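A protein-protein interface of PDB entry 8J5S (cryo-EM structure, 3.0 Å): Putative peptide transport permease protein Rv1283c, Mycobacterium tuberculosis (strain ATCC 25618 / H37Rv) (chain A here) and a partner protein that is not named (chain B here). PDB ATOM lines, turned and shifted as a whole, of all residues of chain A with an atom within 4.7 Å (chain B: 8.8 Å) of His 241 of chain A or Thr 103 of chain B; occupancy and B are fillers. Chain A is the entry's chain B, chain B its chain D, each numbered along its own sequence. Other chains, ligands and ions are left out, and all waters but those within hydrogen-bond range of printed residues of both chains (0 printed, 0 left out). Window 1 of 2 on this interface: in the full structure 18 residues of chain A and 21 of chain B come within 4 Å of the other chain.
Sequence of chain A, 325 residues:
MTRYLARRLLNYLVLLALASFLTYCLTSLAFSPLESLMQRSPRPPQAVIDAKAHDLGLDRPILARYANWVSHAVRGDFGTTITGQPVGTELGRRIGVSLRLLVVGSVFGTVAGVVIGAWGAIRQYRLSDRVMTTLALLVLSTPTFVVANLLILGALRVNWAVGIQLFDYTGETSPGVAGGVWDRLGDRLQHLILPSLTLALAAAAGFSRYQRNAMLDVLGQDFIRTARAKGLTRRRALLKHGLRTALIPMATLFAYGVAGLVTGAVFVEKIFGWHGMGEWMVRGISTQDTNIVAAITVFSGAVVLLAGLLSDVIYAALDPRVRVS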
ATOM      1  N   PHE A 223      18.753 -29.779  30.104  1.00  0.00           N
ATOM      2  CA  PHE A 223      19.963 -29.256  29.490  1.00  0.00           C
ATOM      3  C   PHE A 223      20.480 -30.129  28.363  1.00  0.00           C
ATOM      4  O   PHE A 223      21.206 -29.631  27.503  1.00  0.00           O
ATOM      5  CB  PHE A 223      21.064 -29.037  30.536  1.00  0.00           C
ATOM      6  CG  PHE A 223      21.543 -30.282  31.219  1.00  0.00           C
ATOM      7  CD1 PHE A 223      21.243 -30.508  32.541  1.00  0.00           C
ATOM      8  CD2 PHE A 223      22.342 -31.192  30.565  1.00  0.00           C
ATOM      9  CE1 PHE A 223      21.690 -31.629  33.174  1.00  0.00           C
ATOM     10  CE2 PHE A 223      22.786 -32.313  31.197  1.00  0.00           C
ATOM     11  CZ  PHE A 223      22.462 -32.532  32.499  1.00  0.00           C
ATOM     12  N   ALA A 227      21.532 -28.848  24.726  1.00  0.00           N
ATOM     13  CA  ALA A 227      22.754 -29.301  24.076  1.00  0.00           C
ATOM     14  C   ALA A 227      22.489 -29.774  22.657  1.00  0.00           C
ATOM     15  O   ALA A 227      23.284 -29.514  21.756  1.00  0.00           O
ATOM     16  CB  ALA A 227      23.399 -30.412  24.894  1.00  0.00           C
ATOM     17  N   LEU A 232      24.122 -30.790  18.292  1.00  0.00           N
ATOM     18  CA  LEU A 232      24.742 -32.002  18.802  1.00  0.00           C
ATOM     19  C   LEU A 232      23.756 -33.148  18.651  1.00  0.00           C
ATOM     20  O   LEU A 232      22.660 -33.097  19.206  1.00  0.00           O
ATOM     21  CB  LEU A 232      25.148 -31.835  20.264  1.00  0.00           C
ATOM     22  CG  LEU A 232      26.531 -31.275  20.572  1.00  0.00           C
ATOM     23  CD1 LEU A 232      26.583 -29.802  20.278  1.00  0.00           C
ATOM     24  CD2 LEU A 232      26.876 -31.524  22.015  1.00  0.00           C
ATOM     25  N   ARG A 236      25.725 -38.002  20.865  1.00  0.00           N
ATOM     26  CA  ARG A 236      26.823 -37.195  21.371  1.00  0.00           C
ATOM     27  C   ARG A 236      26.371 -36.321  22.523  1.00  0.00           C
ATOM     28  O   ARG A 236      27.123 -36.106  23.475  1.00  0.00           O
ATOM     29  CB  ARG A 236      27.402 -36.337  20.254  1.00  0.00           C
ATOM     30  CG  ARG A 236      28.600 -35.550  20.685  1.00  0.00           C
ATOM     31  CD  ARG A 236      29.137 -34.694  19.569  1.00  0.00           C
ATOM     32  NE  ARG A 236      30.311 -33.945  20.003  1.00  0.00           N
ATOM     33  CZ  ARG A 236      31.560 -34.294  19.722  1.00  0.00           C
ATOM     34  NH1 ARG A 236      31.802 -35.380  18.999  1.00  0.00           N
ATOM     35  NH2 ARG A 236      32.567 -33.554  20.160  1.00  0.00           N
ATOM     36  N   ALA A 237      25.150 -35.793  22.455  1.00  0.00           N
ATOM     37  CA  ALA A 237      24.641 -34.984  23.553  1.00  0.00           C
ATOM     38  C   ALA A 237      24.580 -35.791  24.837  1.00  0.00           C
ATOM     39  O   ALA A 237      25.075 -35.352  25.877  1.00  0.00           O
ATOM     40  CB  ALA A 237      23.268 -34.425  23.203  1.00  0.00           C
ATOM     41  N   LEU A 238      24.000 -36.991  24.776  1.00  0.00           N
ATOM     42  CA  LEU A 238      23.946 -37.841  25.961  1.00  0.00           C
ATOM     43  C   LEU A 238      25.337 -38.088  26.512  1.00  0.00           C
ATOM     44  O   LEU A 238      25.610 -37.771  27.671  1.00  0.00           O
ATOM     45  CB  LEU A 238      23.278 -39.177  25.652  1.00  0.00           C
ATOM     46  CG  LEU A 238      21.862 -39.271  25.117  1.00  0.00           C
ATOM     47  CD1 LEU A 238      21.736 -40.553  24.322  1.00  0.00           C
ATOM     48  CD2 LEU A 238      20.863 -39.253  26.237  1.00  0.00           C
ATOM     49  N   LEU A 239      26.251 -38.566  25.666  1.00  0.00           N
ATOM     50  CA  LEU A 239      27.576 -38.938  26.151  1.00  0.00           C
ATOM     51  C   LEU A 239      28.313 -37.746  26.743  1.00  0.00           C
ATOM     52  O   LEU A 239      28.865 -37.828  27.842  1.00  0.00           O
ATOM     53  CB  LEU A 239      28.390 -39.560  25.020  1.00  0.00           C
ATOM     54  CG  LEU A 239      27.909 -40.926  24.542  1.00  0.00           C
ATOM     55  CD1 LEU A 239      28.957 -41.576  23.663  1.00  0.00           C
ATOM     56  CD2 LEU A 239      27.561 -41.818  25.720  1.00  0.00           C
ATOM     57  N   LYS A 240      28.317 -36.620  26.035  1.00  0.00           N
ATOM     58  CA  LYS A 240      29.134 -35.483  26.426  1.00  0.00           C
ATOM     59  C   LYS A 240      28.561 -34.723  27.608  1.00  0.00           C
ATOM     60  O   LYS A 240      29.327 -34.163  28.393  1.00  0.00           O
ATOM     61  CB  LYS A 240      29.307 -34.545  25.237  1.00  0.00           C
ATOM     62  CG  LYS A 240      30.537 -33.673  25.298  1.00  0.00           C
ATOM     63  CD  LYS A 240      30.592 -32.736  24.107  1.00  0.00           C
ATOM     64  CE  LYS A 240      31.928 -32.047  23.997  1.00  0.00           C
ATOM     65  NZ  LYS A 240      32.052 -30.946  24.977  1.00  0.00           N
ATOM     66  N   HIS A 241      27.239 -34.672  27.764  1.00  0.00           N
ATOM     67  CA  HIS A 241      26.631 -33.883  28.821  1.00  0.00           C
ATOM     68  C   HIS A 241      25.940 -34.743  29.868  1.00  0.00           C
ATOM     69  O   HIS A 241      26.280 -34.673  31.050  1.00  0.00           O
ATOM     70  CB  HIS A 241      25.639 -32.888  28.207  1.00  0.00           C
ATOM     71  CG  HIS A 241      26.283 -31.819  27.379  1.00  0.00           C
ATOM     72  ND1 HIS A 241      26.450 -30.530  27.830  1.00  0.00           N
ATOM     73  CD2 HIS A 241      26.809 -31.850  26.135  1.00  0.00           C
ATOM     74  CE1 HIS A 241      27.049 -29.815  26.897  1.00  0.00           C
ATOM     75  NE2 HIS A 241      27.275 -30.592  25.858  1.00  0.00           N
ATOM     76  N   GLY A 242      24.989 -35.579  29.461  1.00  0.00           N
ATOM     77  CA  GLY A 242      24.159 -36.253  30.439  1.00  0.00           C
ATOM     78  C   GLY A 242      24.915 -37.316  31.205  1.00  0.00           C
ATOM     79  O   GLY A 242      24.802 -37.414  32.425  1.00  0.00           O
ATOM     80  N   LEU A 243      25.693 -38.131  30.500  1.00  0.00           N
ATOM     81  CA  LEU A 243      26.455 -39.170  31.179  1.00  0.00           C
ATOM     82  C   LEU A 243      27.557 -38.569  32.032  1.00  0.00           C
ATOM     83  O   LEU A 243      27.823 -39.043  33.140  1.00  0.00           O
ATOM     84  CB  LEU A 243      27.036 -40.144  30.161  1.00  0.00           C
ATOM     85  CG  LEU A 243      27.627 -41.427  30.730  1.00  0.00           C
ATOM     86  CD1 LEU A 243      26.734 -42.002  31.806  1.00  0.00           C
ATOM     87  CD2 LEU A 243      27.837 -42.427  29.622  1.00  0.00           C
ATOM     88  N   ARG A 244      28.208 -37.520  31.537  1.00  0.00           N
ATOM     89  CA  ARG A 244      29.249 -36.866  32.312  1.00  0.00           C
ATOM     90  C   ARG A 244      28.686 -36.273  33.593  1.00  0.00           C
ATOM     91  O   ARG A 244      29.346 -36.288  34.634  1.00  0.00           O
ATOM     92  CB  ARG A 244      29.923 -35.790  31.471  1.00  0.00           C
ATOM     93  CG  ARG A 244      31.078 -35.117  32.152  1.00  0.00           C
ATOM     94  CD  ARG A 244      31.955 -34.431  31.150  1.00  0.00           C
ATOM     95  NE  ARG A 244      33.090 -33.781  31.780  1.00  0.00           N
ATOM     96  CZ  ARG A 244      34.190 -33.431  31.134  1.00  0.00           C
ATOM     97  NH1 ARG A 244      34.302 -33.671  29.836  1.00  0.00           N
ATOM     98  NH2 ARG A 244      35.179 -32.845  31.784  1.00  0.00           N
ATOM     99  N   THR A 245      27.469 -35.741  33.538  1.00  0.00           N
ATOM    100  CA  THR A 245      26.842 -35.207  34.738  1.00  0.00           C
ATOM    101  C   THR A 245      26.312 -36.302  35.654  1.00  0.00           C
ATOM    102  O   THR A 245      26.315 -36.137  36.875  1.00  0.00           O
ATOM    103  CB  THR A 245      25.716 -34.258  34.348  1.00  0.00           C
ATOM    104  OG1 THR A 245      26.249 -33.204  33.541  1.00  0.00           O
ATOM    105  CG2 THR A 245      25.070 -33.665  35.574  1.00  0.00           C
ATOM    106  N   MET B  99      16.092 -22.475  33.960  1.00  0.00           N
ATOM    107  CA  MET B  99      16.670 -22.692  35.275  1.00  0.00           C
ATOM    108  C   MET B  99      17.459 -23.985  35.361  1.00  0.00           C
ATOM    109  O   MET B  99      18.176 -24.194  36.343  1.00  0.00           O
ATOM    110  CB  MET B  99      15.581 -22.681  36.346  1.00  0.00           C
ATOM    111  CG  MET B  99      16.053 -22.156  37.693  1.00  0.00           C
ATOM    112  SD  MET B  99      16.797 -20.504  37.647  1.00  0.00           S
ATOM    113  CE  MET B  99      15.604 -19.588  36.677  1.00  0.00           C
ATOM    114  N   SER B 100      17.337 -24.857  34.363  1.00  0.00           N
ATOM    115  CA  SER B 100      18.150 -26.060  34.266  1.00  0.00           C
ATOM    116  C   SER B 100      18.549 -26.327  32.828  1.00  0.00           C
ATOM    117  O   SER B 100      18.770 -27.478  32.451  1.00  0.00           O
ATOM    118  CB  SER B 100      17.418 -27.270  34.831  1.00  0.00           C
ATOM    119  OG  SER B 100      16.429 -27.718  33.930  1.00  0.00           O
ATOM    120  N   ALA B 101      18.642 -25.283  32.015  1.00  0.00           N
ATOM    121  CA  ALA B 101      18.901 -25.420  30.591  1.00  0.00           C
ATOM    122  C   ALA B 101      20.377 -25.411  30.247  1.00  0.00           C
ATOM    123  O   ALA B 101      20.717 -25.449  29.065  1.00  0.00           O
ATOM    124  CB  ALA B 101      18.201 -24.309  29.817  1.00  0.00           C
ATOM    125  N   LEU B 102      21.256 -25.354  31.236  1.00  0.00           N
ATOM    126  CA  LEU B 102      22.691 -25.317  31.014  1.00  0.00           C
ATOM    127  C   LEU B 102      23.343 -26.482  31.738  1.00  0.00           C
ATOM    128  O   LEU B 102      22.939 -26.832  32.846  1.00  0.00           O
ATOM    129  CB  LEU B 102      23.283 -23.997  31.496  1.00  0.00           C
ATOM    130  CG  LEU B 102      22.729 -22.725  30.862  1.00  0.00           C
ATOM    131  CD1 LEU B 102      23.088 -21.533  31.698  1.00  0.00           C
ATOM    132  CD2 LEU B 102      23.258 -22.556  29.463  1.00  0.00           C
ATOM    133  N   THR B 103      24.340 -27.085  31.108  1.00  0.00           N
ATOM    134  CA  THR B 103      25.043 -28.201  31.722  1.00  0.00           C
ATOM    135  C   THR B 103      25.800 -27.699  32.937  1.00  0.00           C
ATOM    136  O   THR B 103      26.591 -26.761  32.813  1.00  0.00           O
ATOM    137  CB  THR B 103      26.008 -28.854  30.744  1.00  0.00           C
ATOM    138  OG1 THR B 103      25.343 -29.105  29.503  1.00  0.00           O
ATOM    139  CG2 THR B 103      26.508 -30.157  31.300  1.00  0.00           C
ATOM    140  N   PRO B 104      25.593 -28.276  34.119  1.00  0.00           N
ATOM    141  CA  PRO B 104      26.228 -27.724  35.321  1.00  0.00           C
ATOM    142  C   PRO B 104      27.736 -27.890  35.367  1.00  0.00           C
ATOM    143  O   PRO B 104      28.390 -27.145  36.102  1.00  0.00           O
ATOM    144  CB  PRO B 104      25.547 -28.493  36.455  1.00  0.00           C
ATOM    145  CG  PRO B 104      25.050 -29.733  35.828  1.00  0.00           C
ATOM    146  CD  PRO B 104      24.684 -29.385  34.434  1.00  0.00           C
ATOM    147  N   VAL B 105      28.312 -28.820  34.613  1.00  0.00           N
ATOM    148  CA  VAL B 105      29.727 -29.142  34.726  1.00  0.00           C
ATOM    149  C   VAL B 105      30.554 -28.453  33.641  1.00  0.00           C
ATOM    150  O   VAL B 105      31.701 -28.825  33.417  1.00  0.00           O
ATOM    151  CB  VAL B 105      29.962 -30.657  34.716  1.00  0.00           C
ATOM    152  CG1 VAL B 105      29.150 -31.316  35.795  1.00  0.00           C
ATOM    153  CG2 VAL B 105      29.608 -31.238  33.373  1.00  0.00           C
ATOM    154  N   TYR B 106      29.995 -27.457  32.968  1.00  0.00           N
ATOM    155  CA  TYR B 106      30.708 -26.744  31.920  1.00  0.00           C
ATOM    156  C   TYR B 106      30.655 -25.250  32.179  1.00  0.00           C
ATOM    157  O   TYR B 106      29.624 -24.715  32.582  1.00  0.00           O
ATOM    158  CB  TYR B 106      30.125 -27.037  30.543  1.00  0.00           C
ATOM    159  CG  TYR B 106      30.497 -28.378  29.968  1.00  0.00           C
ATOM    160  CD1 TYR B 106      31.627 -28.532  29.199  1.00  0.00           C
ATOM    161  CD2 TYR B 106      29.707 -29.487  30.187  1.00  0.00           C
ATOM    162  CE1 TYR B 106      31.963 -29.755  28.670  1.00  0.00           C
ATOM    163  CE2 TYR B 106      30.038 -30.710  29.664  1.00  0.00           C
ATOM    164  CZ  TYR B 106      31.163 -30.838  28.906  1.00  0.00           C
ATOM    165  OH  TYR B 106      31.488 -32.060  28.383  1.00  0.00           O
ATOM    166  N   THR B 107      31.775 -24.584  31.945  1.00  0.00           N
ATOM    167  CA  THR B 107      31.833 -23.135  32.039  1.00  0.00           C
ATOM    168  C   THR B 107      30.981 -22.510  30.945  1.00  0.00           C
ATOM    169  O   THR B 107      30.951 -23.000  29.816  1.00  0.00           O
ATOM    170  CB  THR B 107      33.278 -22.676  31.915  1.00  0.00           C
ATOM    171  OG1 THR B 107      34.005 -23.082  33.074  1.00  0.00           O
ATOM    172  CG2 THR B 107      33.359 -21.207  31.793  1.00  0.00           C
ATOM    173  N   VAL B 108      30.288 -21.419  31.277  1.00  0.00           N
ATOM    174  CA  VAL B 108      29.335 -20.839  30.334  1.00  0.00           C
ATOM    175  C   VAL B 108      30.033 -20.398  29.053  1.00  0.00           C
ATOM    176  O   VAL B 108      29.481 -20.526  27.956  1.00  0.00           O
ATOM    177  CB  VAL B 108      28.548 -19.691  30.991  1.00  0.00           C
ATOM    178  CG1 VAL B 108      27.882 -20.174  32.252  1.00  0.00           C
ATOM    179  CG2 VAL B 108      29.436 -18.523  31.294  1.00  0.00           C
ATOM    180  N   ASP B 110      32.652 -21.834  27.700  1.00  0.00           N
ATOM    181  CA  ASP B 110      32.927 -23.053  26.956  1.00  0.00           C
ATOM    182  C   ASP B 110      31.666 -23.819  26.586  1.00  0.00           C
ATOM    183  O   ASP B 110      31.771 -24.926  26.059  1.00  0.00           O
ATOM    184  CB  ASP B 110      33.879 -23.946  27.746  1.00  0.00           C
ATOM    185  CG  ASP B 110      35.319 -23.467  27.674  1.00  0.00           C
ATOM    186  OD1 ASP B 110      36.237 -24.303  27.790  1.00  0.00           O
ATOM    187  OD2 ASP B 110      35.535 -22.252  27.498  1.00  0.00           O
ATOM    188  N   GLN B 111      30.484 -23.269  26.856  1.00  0.00           N
ATOM    189  CA  GLN B 111      29.233 -23.731  26.264  1.00  0.00           C
ATOM    190  C   GLN B 111      28.828 -22.876  25.073  1.00  0.00           C
ATOM    191  O   GLN B 111      28.529 -23.399  23.994  1.00  0.00           O
ATOM    192  CB  GLN B 111      28.121 -23.722  27.311  1.00  0.00           C
ATOM    193  CG  GLN B 111      28.417 -24.544  28.530  1.00  0.00           C
ATOM    194  CD  GLN B 111      27.175 -24.985  29.249  1.00  0.00           C
ATOM    195  OE1 GLN B 111      26.260 -25.518  28.642  1.00  0.00           O
ATOM    196  NE2 GLN B 111      27.135 -24.771  30.547  1.00  0.00           N
ATOM    197  N   ILE B 112      28.825 -21.555  25.247  1.00  0.00           N
ATOM    198  CA  ILE B 112      28.635 -20.653  24.120  1.00  0.00           C
ATOM    199  C   ILE B 112      29.725 -20.810  23.077  1.00  0.00           C
ATOM    200  O   ILE B 112      29.598 -20.274  21.976  1.00  0.00           O
ATOM    201  CB  ILE B 112      28.565 -19.190  24.600  1.00  0.00           C
ATOM    202  CG1 ILE B 112      27.722 -19.085  25.861  1.00  0.00           C
ATOM    203  CG2 ILE B 112      27.955 -18.304  23.550  1.00  0.00           C
ATOM    204  CD1 ILE B 112      27.525 -17.676  26.331  1.00  0.00           C
ATOM    205  N   GLU B 114      31.191 -24.211  22.491  1.00  0.00           N
ATOM    206  CA  GLU B 114      30.855 -25.466  21.827  1.00  0.00           C
ATOM    207  C   GLU B 114      29.761 -25.232  20.799  1.00  0.00           C
ATOM    208  O   GLU B 114      29.806 -25.785  19.695  1.00  0.00           O
ATOM    209  CB  GLU B 114      30.447 -26.533  22.846  1.00  0.00           C
ATOM    210  CG  GLU B 114      29.027 -26.437  23.315  1.00  0.00           C
ATOM    211  CD  GLU B 114      28.525 -27.664  24.044  1.00  0.00           C
ATOM    212  OE1 GLU B 114      27.349 -27.650  24.470  1.00  0.00           O
ATOM    213  OE2 GLU B 114      29.290 -28.633  24.192  1.00  0.00           O
ATOM    214  N   ALA B 115      28.811 -24.352  21.116  1.00  0.00           N
ATOM    215  CA  ALA B 115      27.790 -23.987  20.142  1.00  0.00           C
ATOM    216  C   ALA B 115      28.415 -23.463  18.860  1.00  0.00           C
ATOM    217  O   ALA B 115      28.027 -23.864  17.761  1.00  0.00           O
ATOM    218  CB  ALA B 115      26.849 -22.945  20.734  1.00  0.00           C
ATOM    219  N   VAL B 118      30.541 -26.232  16.779  1.00  0.00           N
ATOM    220  CA  VAL B 118      29.924 -27.386  16.114  1.00  0.00           C
ATOM    221  C   VAL B 118      29.699 -27.142  14.622  1.00  0.00           C
ATOM    222  O   VAL B 118      29.970 -28.016  13.801  1.00  0.00           O
ATOM    223  CB  VAL B 118      28.614 -27.795  16.804  1.00  0.00           C
ATOM    224  CG1 VAL B 118      28.084 -29.045  16.160  1.00  0.00           C
ATOM    225  CG2 VAL B 118      28.865 -28.092  18.233  1.00  0.00           C
ATOM    226  N   ALA B 150      32.566 -18.719  34.720  1.00  0.00           N
ATOM    227  CA  ALA B 150      31.684 -19.102  35.805  1.00  0.00           C
ATOM    228  C   ALA B 150      30.822 -20.282  35.400  1.00  0.00           C
ATOM    229  O   ALA B 150      30.448 -20.429  34.239  1.00  0.00           O
ATOM    230  CB  ALA B 150      30.791 -17.936  36.220  1.00  0.00           C
ATOM    231  N   PHE B 151      30.522 -21.110  36.353  1.00  0.00           N
ATOM    232  CA  PHE B 151      29.651 -22.245  36.127  1.00  0.00           C
ATOM    233  C   PHE B 151      28.201 -21.830  36.312  1.00  0.00           C
ATOM    234  O   PHE B 151      27.915 -20.832  36.970  1.00  0.00           O
ATOM    235  CB  PHE B 151      30.025 -23.378  37.075  1.00  0.00           C
ATOM    236  CG  PHE B 151      31.379 -23.961  36.800  1.00  0.00           C
ATOM    237  CD1 PHE B 151      32.515 -23.339  37.249  1.00  0.00           C
ATOM    238  CD2 PHE B 151      31.510 -25.122  36.076  1.00  0.00           C
ATOM    239  CE1 PHE B 151      33.747 -23.864  36.986  1.00  0.00           C
ATOM    240  CE2 PHE B 151      32.743 -25.645  35.811  1.00  0.00           C
ATOM    241  CZ  PHE B 151      33.861 -25.015  36.266  1.00  0.00           C
ATOM    242  N   PRO B 152      27.255 -22.559  35.721  1.00  0.00           N
ATOM    243  CA  PRO B 152      25.862 -22.094  35.734  1.00  0.00           C
ATOM    244  C   PRO B 152      25.260 -21.938  37.116  1.00  0.00           C
ATOM    245  O   PRO B 152      24.288 -21.193  37.262  1.00  0.00           O
ATOM    246  CB  PRO B 152      25.132 -23.173  34.929  1.00  0.00           C
ATOM    247  CG  PRO B 152      26.163 -23.731  34.048  1.00  0.00           C
ATOM    248  CD  PRO B 152      27.427 -23.720  34.835  1.00  0.00           C
ATOM    249  N   HIS B 153      25.787 -22.613  38.133  1.00  0.00           N
ATOM    250  CA  HIS B 153      25.165 -22.574  39.450  1.00  0.00           C
ATOM    251  C   HIS B 153      25.408 -21.271  40.193  1.00  0.00           C
ATOM    252  O   HIS B 153      24.768 -21.041  41.222  1.00  0.00           O
ATOM    253  CB  HIS B 153      25.653 -23.743  40.306  1.00  0.00           C
ATOM    254  CG  HIS B 153      27.121 -23.721  40.578  1.00  0.00           C
ATOM    255  ND1 HIS B 153      27.645 -23.390  41.807  1.00  0.00           N
ATOM    256  CD2 HIS B 153      28.178 -23.993  39.781  1.00  0.00           C
ATOM    257  CE1 HIS B 153      28.963 -23.453  41.753  1.00  0.00           C
ATOM    258  NE2 HIS B 153      29.311 -23.814  40.533  1.00  0.00           N
ATOM    259  N   LEU B 155      24.977 -18.142  38.813  1.00  0.00           N
ATOM    260  CA  LEU B 155      24.384 -17.113  37.976  1.00  0.00           C
ATOM    261  C   LEU B 155      23.035 -16.697  38.543  1.00  0.00           C
ATOM    262  O   LEU B 155      22.359 -17.476  39.216  1.00  0.00           O
ATOM    263  CB  LEU B 155      24.224 -17.592  36.541  1.00  0.00           C
ATOM    264  CG  LEU B 155      25.516 -17.799  35.760  1.00  0.00           C
ATOM    265  CD1 LEU B 155      25.222 -18.432  34.421  1.00  0.00           C
ATOM    266  CD2 LEU B 155      26.234 -16.493  35.573  1.00  0.00           C
ATOM    267  N   ARG B 160      21.562 -16.423  33.525  1.00  0.00           N
ATOM    268  CA  ARG B 160      21.459 -17.672  32.790  1.00  0.00           C
ATOM    269  C   ARG B 160      20.247 -17.682  31.879  1.00  0.00           C
ATOM    270  O   ARG B 160      20.173 -18.521  30.981  1.00  0.00           O
ATOM    271  CB  ARG B 160      21.422 -18.855  33.748  1.00  0.00           C
ATOM    272  CG  ARG B 160      20.367 -18.762  34.789  1.00  0.00           C
ATOM    273  CD  ARG B 160      19.912 -20.125  35.209  1.00  0.00           C
ATOM    274  NE  ARG B 160      20.924 -20.831  35.980  1.00  0.00           N
ATOM    275  CZ  ARG B 160      20.905 -20.934  37.302  1.00  0.00           C
ATOM    276  NH1 ARG B 160      21.856 -21.600  37.931  1.00  0.00           N
ATOM    277  NH2 ARG B 160      19.928 -20.374  37.993  1.00  0.00           N
ATOM    278  N   VAL B 163      22.355 -16.219  28.929  1.00  0.00           N
ATOM    279  CA  VAL B 163      23.312 -17.135  28.322  1.00  0.00           C
ATOM    280  C   VAL B 163      22.626 -17.993  27.270  1.00  0.00           C
ATOM    281  O   VAL B 163      23.225 -18.329  26.242  1.00  0.00           O
ATOM    282  CB  VAL B 163      23.994 -17.997  29.398  1.00  0.00           C
ATOM    283  CG1 VAL B 163      25.062 -18.856  28.779  1.00  0.00           C
ATOM    284  CG2 VAL B 163      24.606 -17.126  30.455  1.00  0.00           C
ATOM    285  N   VAL B 164      21.367 -18.355  27.499  1.00  0.00           N
ATOM    286  CA  VAL B 164      20.619 -19.129  26.515  1.00  0.00           C
ATOM    287  C   VAL B 164      20.427 -18.325  25.238  1.00  0.00           C
ATOM    288  O   VAL B 164      20.527 -18.861  24.131  1.00  0.00           O
ATOM    289  CB  VAL B 164      19.275 -19.578  27.109  1.00  0.00           C
ATOM    290  CG1 VAL B 164      18.551 -20.474  26.142  1.00  0.00           C
ATOM    291  CG2 VAL B 164      19.507 -20.292  28.409  1.00  0.00           C
ATOM    292  N   ILE B 167      23.701 -18.370  23.362  1.00  0.00           N
ATOM    293  CA  ILE B 167      23.888 -19.647  22.678  1.00  0.00           C
ATOM    294  C   ILE B 167      23.029 -19.706  21.423  1.00  0.00           C
ATOM    295  O   ILE B 167      23.490 -20.126  20.357  1.00  0.00           O
ATOM    296  CB  ILE B 167      23.570 -20.812  23.631  1.00  0.00           C
ATOM    297  CG1 ILE B 167      24.758 -21.120  24.523  1.00  0.00           C
ATOM    298  CG2 ILE B 167      23.198 -22.039  22.861  1.00  0.00           C
ATOM    299  CD1 ILE B 167      24.409 -21.972  25.708  1.00  0.00           C
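The side-chain carboxylate of Glu 114 of chain B is in salt-bridge range of the side-chain amino group of Lys 240 of chain A (3.7 Å). N of Phe 223 of chain A sits at hydrogen-bond distance from O of Ser 100 of chain B (3.3 Å). ND1 of His 241 of chain A lies within hydrogen-bond range of OG1 of Thr 103 of chain B, 2.5 Å away. A ring nitrogen (NE2) of His 241 of chain A is in hydrogen-bond range of the side-chain carboxylate (OE1) of Glu 114 of chain B (3.3 Å). The side-chain hydroxyl (OH) of Tyr 106 of chain B sits at hydrogen-bond distance from the backbone carbonyl oxygen (O) of Lys 240 of chain A (3.0 Å).
The side-chain amide nitrogen of Gln 111 of chain B is in hydrogen-bond range of the backbone carbonyl oxygen of Thr 103 of chain B (3.1 Å). NE2 of Gln 111 of chain B sits at hydrogen-bond distance from O of Tyr 106 of chain B (3.2 Å). O of His 241 of chain A sits at hydrogen-bond distance from OG1 of Thr 245 of chain A.
CB of Phe 223 of chain A touches C of Ala 101 of chain B, 3.7 Å away. Phe 223 of chain A touches Leu 102 of chain B. Phe 223 of chain A touches Thr 103 of chain B (CD2 to OG1, 3.8 Å). Phe 223 of chain A touches Pro 104 of chain B (CE1 to CD, 3.9 Å). CD1 of Leu 232 of chain A touches CG2 of Val 118 of chain B, 3.5 Å away. Tyr 106 of chain B touches Arg 244 of chain A. Thr 245 of chain A touches Thr 103 of chain B. Thr 245 of chain A touches Pro 104 of chain B (CG2 to CG, 3.9 Å). OG1 of Thr 245 of chain A touches CG2 of Val 105 of chain B, at 3.9 Å.
Of the printed residues of chain B, Leu 232 of chain A touches Val 118. Arg 236 of chain A touches none of the printed residues of chain B. Of the printed residues of chain A, Ser 100 of chain B touches Phe 223. Of the printed residues of chain A, Leu 102 of chain B touches Phe 223 (3.6 Å). Of chain A, only Phe 223 (3.8 Å), His 241 (2.5 Å) and Thr 245 (3.8 Å) come within 4 Å of Thr 103 of chain B. Printed residues of chain A within 4 Å of Pro 104 of chain B: Phe 223 (3.9 Å) and Thr 245 (3.9 Å). Ile 112 of chain B touches none of the printed residues of chain A. Printed residues of chain A within 4 Å of Glu 114 of chain B: Lys 240 and His 241. The nearest residue of chain B that does not touch His 241 of chain A is Tyr 106 of chain B (4.03 Å). The nearest printed residue of chain A that does not touch Thr 103 of chain B is Ala 227 of chain A (5.2 Å).
Of the 13 printed residues of chain A, 6 touch a printed residue of chain B. Printed residues of chain A that touch a printed residue of chain B: Phe 223, Leu 232, Lys 240, His 241, Arg 244 and Thr 245. Hydrophobic or aromatic side chains of chain A that line the printed part of chain B: Phe 223, Leu 232 and His 241. Hydrophobic or aromatic side chains of chain B that line the printed part of chain A: Pro 104, Val 105, Tyr 106 and Val 118. Among the printed residues, 14 pairs touch across the chains.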
